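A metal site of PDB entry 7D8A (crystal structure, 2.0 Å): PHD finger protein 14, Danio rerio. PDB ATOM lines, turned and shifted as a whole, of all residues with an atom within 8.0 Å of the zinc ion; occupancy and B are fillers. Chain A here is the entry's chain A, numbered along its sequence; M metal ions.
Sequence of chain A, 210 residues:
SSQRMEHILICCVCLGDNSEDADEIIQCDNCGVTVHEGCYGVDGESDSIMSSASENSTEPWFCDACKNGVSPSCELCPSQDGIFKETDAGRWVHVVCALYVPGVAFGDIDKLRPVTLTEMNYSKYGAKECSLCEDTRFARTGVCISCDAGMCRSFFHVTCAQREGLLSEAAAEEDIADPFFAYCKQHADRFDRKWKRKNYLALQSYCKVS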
ATOM      1  N   ILE A  10      25.146  24.367  -7.547  1.00  0.00           N
ATOM      2  CA  ILE A  10      25.505  23.983  -8.911  1.00  0.00           C
ATOM      3  C   ILE A  10      24.233  23.945  -9.735  1.00  0.00           C
ATOM      4  O   ILE A  10      23.202  23.420  -9.282  1.00  0.00           O
ATOM      5  CB  ILE A  10      26.238  22.632  -8.915  1.00  0.00           C
ATOM      6  CG1 ILE A  10      27.618  22.839  -8.284  1.00  0.00           C
ATOM      7  CG2 ILE A  10      26.334  22.055 -10.352  1.00  0.00           C
ATOM      8  CD1 ILE A  10      28.261  21.601  -7.840  1.00  0.00           C
ATOM      9  N   CYS A  11      24.289  24.523 -10.929  1.00  0.00           N
ATOM     10  CA  CYS A  11      23.157  24.525 -11.837  1.00  0.00           C
ATOM     11  C   CYS A  11      23.030  23.165 -12.517  1.00  0.00           C
ATOM     12  O   CYS A  11      23.988  22.666 -13.120  1.00  0.00           O
ATOM     13  CB  CYS A  11      23.337  25.628 -12.883  1.00  0.00           C
ATOM     14  SG  CYS A  11      22.148  25.529 -14.264  1.00  0.00           S
ATOM     15  N   CYS A  12      21.856  22.544 -12.410  1.00  0.00           N
ATOM     16  CA  CYS A  12      21.679  21.201 -12.959  1.00  0.00           C
ATOM     17  C   CYS A  12      21.570  21.173 -14.478  1.00  0.00           C
ATOM     18  O   CYS A  12      21.391  20.087 -15.044  1.00  0.00           O
ATOM     19  CB  CYS A  12      20.437  20.527 -12.352  1.00  0.00           C
ATOM     20  SG  CYS A  12      18.857  21.205 -12.913  1.00  0.00           S
ATOM     21  N   VAL A  13      21.610  22.310 -15.155  1.00  0.00           N
ATOM     22  CA  VAL A  13      21.562  22.336 -16.620  1.00  0.00           C
ATOM     23  C   VAL A  13      22.954  22.445 -17.216  1.00  0.00           C
ATOM     24  O   VAL A  13      23.345  21.616 -18.035  1.00  0.00           O
ATOM     25  CB  VAL A  13      20.653  23.488 -17.117  1.00  0.00           C
ATOM     26  CG1 VAL A  13      20.741  23.609 -18.625  1.00  0.00           C
ATOM     27  CG2 VAL A  13      19.191  23.229 -16.709  1.00  0.00           C
ATOM     28  N   CYS A  14      23.726  23.440 -16.806  1.00  0.00           N
ATOM     29  CA  CYS A  14      25.057  23.654 -17.345  1.00  0.00           C
ATOM     30  C   CYS A  14      26.177  23.181 -16.421  1.00  0.00           C
ATOM     31  O   CYS A  14      27.332  23.192 -16.843  1.00  0.00           O
ATOM     32  CB  CYS A  14      25.263  25.141 -17.678  1.00  0.00           C
ATOM     33  SG  CYS A  14      25.488  26.219 -16.235  1.00  0.00           S
ATOM     34  N   LEU A  15      25.862  22.784 -15.190  1.00  0.00           N
ATOM     35  CA  LEU A  15      26.811  22.354 -14.161  1.00  0.00           C
ATOM     36  C   LEU A  15      27.763  23.453 -13.725  1.00  0.00           C
ATOM     37  O   LEU A  15      28.800  23.161 -13.123  1.00  0.00           O
ATOM     38  CB  LEU A  15      27.620  21.123 -14.595  1.00  0.00           C
ATOM     39  CG  LEU A  15      26.824  19.878 -14.980  1.00  0.00           C
ATOM     40  CD1 LEU A  15      27.771  18.853 -15.588  1.00  0.00           C
ATOM     41  CD2 LEU A  15      26.067  19.273 -13.800  1.00  0.00           C
ATOM     42  N   GLY A  16      27.457  24.718 -14.015  1.00  0.00           N
ATOM     43  CA  GLY A  16      28.300  25.796 -13.540  1.00  0.00           C
ATOM     44  C   GLY A  16      28.007  26.112 -12.088  1.00  0.00           C
ATOM     45  O   GLY A  16      26.988  25.689 -11.526  1.00  0.00           O
ATOM     46  N   ASP A  17      28.906  26.852 -11.453  1.00  0.00           N
ATOM     47  CA  ASP A  17      28.717  27.188 -10.054  1.00  0.00           C
ATOM     48  C   ASP A  17      28.734  28.685  -9.783  1.00  0.00           C
ATOM     49  O   ASP A  17      28.667  29.080  -8.611  1.00  0.00           O
ATOM     50  CB  ASP A  17      29.751  26.473  -9.176  1.00  0.00           C
ATOM     51  CG  ASP A  17      31.183  26.884  -9.487  1.00  0.00           C
ATOM     52  OD1 ASP A  17      31.411  27.676 -10.430  1.00  0.00           O
ATOM     53  OD2 ASP A  17      32.096  26.384  -8.797  1.00  0.00           O
ATOM     54  N   ASN A  18      28.798  29.518 -10.813  1.00  0.00           N
ATOM     55  CA  ASN A  18      28.789  30.956 -10.576  1.00  0.00           C
ATOM     56  C   ASN A  18      27.363  31.439 -10.400  1.00  0.00           C
ATOM     57  O   ASN A  18      26.485  31.159 -11.229  1.00  0.00           O
ATOM     58  CB  ASN A  18      29.480  31.707 -11.700  1.00  0.00           C
ATOM     59  CG  ASN A  18      30.116  33.004 -11.205  1.00  0.00           C
ATOM     60  OD1 ASN A  18      29.525  34.088 -11.326  1.00  0.00           O
ATOM     61  ND2 ASN A  18      31.310  32.898 -10.633  1.00  0.00           N
ATOM     62  N   ASP A  23      22.375  36.595 -12.597  1.00  0.00           N
ATOM     63  CA  ASP A  23      22.029  35.203 -12.934  1.00  0.00           C
ATOM     64  C   ASP A  23      22.260  34.352 -11.692  1.00  0.00           C
ATOM     65  O   ASP A  23      23.339  33.799 -11.481  1.00  0.00           O
ATOM     66  CB  ASP A  23      22.840  34.695 -14.127  1.00  0.00           C
ATOM     67  CG  ASP A  23      22.283  33.405 -14.673  1.00  0.00           C
ATOM     68  OD1 ASP A  23      21.167  33.030 -14.269  1.00  0.00           O
ATOM     69  OD2 ASP A  23      22.963  32.762 -15.508  1.00  0.00           O
ATOM     70  N   GLU A  24      21.225  34.242 -10.866  1.00  0.00           N
ATOM     71  CA  GLU A  24      21.343  33.502  -9.618  1.00  0.00           C
ATOM     72  C   GLU A  24      21.077  32.029  -9.857  1.00  0.00           C
ATOM     73  O   GLU A  24      20.255  31.652 -10.690  1.00  0.00           O
ATOM     74  CB  GLU A  24      20.377  34.053  -8.567  1.00  0.00           C
ATOM     75  CG  GLU A  24      20.351  33.261  -7.269  1.00  0.00           C
ATOM     76  CD  GLU A  24      19.463  33.878  -6.192  1.00  0.00           C
ATOM     77  OE1 GLU A  24      18.368  34.392  -6.507  1.00  0.00           O
ATOM     78  OE2 GLU A  24      19.886  33.852  -5.023  1.00  0.00           O
ATOM     79  N   ILE A  25      21.793  31.179  -9.119  1.00  0.00           N
ATOM     80  CA  ILE A  25      21.388  29.777  -9.020  1.00  0.00           C
ATOM     81  C   ILE A  25      20.307  29.696  -7.947  1.00  0.00           C
ATOM     82  O   ILE A  25      20.541  30.037  -6.784  1.00  0.00           O
ATOM     83  CB  ILE A  25      22.571  28.859  -8.698  1.00  0.00           C
ATOM     84  CG1 ILE A  25      23.671  29.042  -9.751  1.00  0.00           C
ATOM     85  CG2 ILE A  25      22.107  27.402  -8.676  1.00  0.00           C
ATOM     86  CD1 ILE A  25      24.979  28.322  -9.421  1.00  0.00           C
ATOM     87  N   THR A  34      18.316  22.672  -8.453  1.00  0.00           N
ATOM     88  CA  THR A  34      18.981  23.965  -8.489  1.00  0.00           C
ATOM     89  C   THR A  34      19.369  24.301  -9.921  1.00  0.00           C
ATOM     90  O   THR A  34      19.863  23.445 -10.665  1.00  0.00           O
ATOM     91  CB  THR A  34      20.225  23.947  -7.574  1.00  0.00           C
ATOM     92  OG1 THR A  34      21.005  22.792  -7.857  1.00  0.00           O
ATOM     93  CG2 THR A  34      19.793  23.915  -6.113  1.00  0.00           C
ATOM     94  N   VAL A  35      19.149  25.556 -10.301  1.00  0.00           N
ATOM     95  CA  VAL A  35      19.307  25.962 -11.701  1.00  0.00           C
ATOM     96  C   VAL A  35      19.633  27.450 -11.759  1.00  0.00           C
ATOM     97  O   VAL A  35      19.128  28.243 -10.958  1.00  0.00           O
ATOM     98  CB  VAL A  35      18.031  25.636 -12.526  1.00  0.00           C
ATOM     99  CG1 VAL A  35      16.825  26.473 -12.036  1.00  0.00           C
ATOM    100  CG2 VAL A  35      18.270  25.813 -14.034  1.00  0.00           C
ATOM    101  N   HIS A  36      20.479  27.830 -12.719  1.00  0.00           N
ATOM    102  CA  HIS A  36      20.612  29.239 -13.073  1.00  0.00           C
ATOM    103  C   HIS A  36      19.254  29.770 -13.535  1.00  0.00           C
ATOM    104  O   HIS A  36      18.582  29.139 -14.364  1.00  0.00           O
ATOM    105  CB  HIS A  36      21.625  29.424 -14.197  1.00  0.00           C
ATOM    106  CG  HIS A  36      23.054  29.474 -13.757  1.00  0.00           C
ATOM    107  ND1 HIS A  36      24.024  28.658 -14.298  1.00  0.00           N
ATOM    108  CD2 HIS A  36      23.691  30.286 -12.875  1.00  0.00           C
ATOM    109  CE1 HIS A  36      25.195  28.950 -13.744  1.00  0.00           C
ATOM    110  NE2 HIS A  36      25.016  29.928 -12.881  1.00  0.00           N
ATOM    111  N   GLU A  37      18.852  30.922 -12.999  1.00  0.00           N
ATOM    112  CA  GLU A  37      17.723  31.656 -13.550  1.00  0.00           C
ATOM    113  C   GLU A  37      17.800  31.727 -15.074  1.00  0.00           C
ATOM    114  O   GLU A  37      16.826  31.443 -15.780  1.00  0.00           O
ATOM    115  CB  GLU A  37      17.695  33.074 -12.968  1.00  0.00           C
ATOM    116  CG  GLU A  37      17.326  33.130 -11.506  1.00  0.00           C
ATOM    117  CD  GLU A  37      17.392  34.539 -10.988  1.00  0.00           C
ATOM    118  OE1 GLU A  37      18.393  35.232 -11.299  1.00  0.00           O
ATOM    119  OE2 GLU A  37      16.442  34.964 -10.281  1.00  0.00           O
ATOM    120  N   GLY A  38      18.984  32.104 -15.593  1.00  0.00           N
ATOM    121  CA  GLY A  38      19.180  32.239 -17.022  1.00  0.00           C
ATOM    122  C   GLY A  38      19.222  30.942 -17.788  1.00  0.00           C
ATOM    123  O   GLY A  38      19.047  30.954 -19.004  1.00  0.00           O
ATOM    124  N   CYS A  39      19.437  29.816 -17.104  1.00  0.00           N
ATOM    125  CA  CYS A  39      19.371  28.507 -17.751  1.00  0.00           C
ATOM    126  C   CYS A  39      17.959  27.931 -17.762  1.00  0.00           C
ATOM    127  O   CYS A  39      17.762  26.823 -18.286  1.00  0.00           O
ATOM    128  CB  CYS A  39      20.327  27.509 -17.068  1.00  0.00           C
ATOM    129  SG  CYS A  39      22.128  27.783 -17.330  1.00  0.00           S
ATOM    130  N   TYR A  40      16.984  28.636 -17.208  1.00  0.00           N
ATOM    131  CA  TYR A  40      15.626  28.118 -17.134  1.00  0.00           C
ATOM    132  C   TYR A  40      14.586  29.105 -17.639  1.00  0.00           C
ATOM    133  O   TYR A  40      13.395  28.802 -17.585  1.00  0.00           O
ATOM    134  CB  TYR A  40      15.303  27.726 -15.688  1.00  0.00           C
ATOM    135  CG  TYR A  40      14.141  26.768 -15.504  1.00  0.00           C
ATOM    136  CD1 TYR A  40      14.124  25.524 -16.117  1.00  0.00           C
ATOM    137  CD2 TYR A  40      13.070  27.093 -14.664  1.00  0.00           C
ATOM    138  CE1 TYR A  40      13.066  24.634 -15.929  1.00  0.00           C
ATOM    139  CE2 TYR A  40      12.021  26.224 -14.464  1.00  0.00           C
ATOM    140  CZ  TYR A  40      12.018  24.994 -15.097  1.00  0.00           C
ATOM    141  OH  TYR A  40      10.955  24.150 -14.886  1.00  0.00           O
ATOM    142  N   GLU A 169      29.497  23.853 -23.827  1.00  0.00           N
ATOM    143  CA  GLU A 169      28.777  24.983 -24.391  1.00  0.00           C
ATOM    144  C   GLU A 169      29.812  25.994 -24.843  1.00  0.00           C
ATOM    145  O   GLU A 169      30.629  26.422 -24.025  1.00  0.00           O
ATOM    146  CB  GLU A 169      27.811  25.602 -23.380  1.00  0.00           C
ATOM    147  CG  GLU A 169      27.000  26.751 -23.963  1.00  0.00           C
ATOM    148  CD  GLU A 169      26.120  27.444 -22.935  1.00  0.00           C
ATOM    149  OE1 GLU A 169      26.123  27.036 -21.750  1.00  0.00           O
ATOM    150  OE2 GLU A 169      25.429  28.399 -23.324  1.00  0.00           O
HETATM  151 ZN    ZN M   1      23.322  26.990 -15.670  1.00  0.00          ZN
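A ring nitrogen (NE2) of His 36 is in hydrogen-bond range of the backbone carbonyl oxygen (O) of Asn 18, 2.5 Å away.
The backbone NH (N) of Val 13 sits close to the side-chain sulfur (SG) of Cys 11, at 3.4 Å.
N of Cys 11 lies within hydrogen-bond range of O of Gly 16 (3.0 Å).
The side-chain sulfur (SG) of Cys 14 lies close to the backbone NH (N) of Gly 16 (3.3 Å).
The zinc ion is bound by the side-chain sulfur (SG) of Cys 39 (2.2 Å), a ring nitrogen (ND1) of His 36 (2.3 Å), the side-chain sulfur (SG) of Cys 11 (2.3 Å) and the side-chain sulfur (SG) of Cys 14 (2.4 Å).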
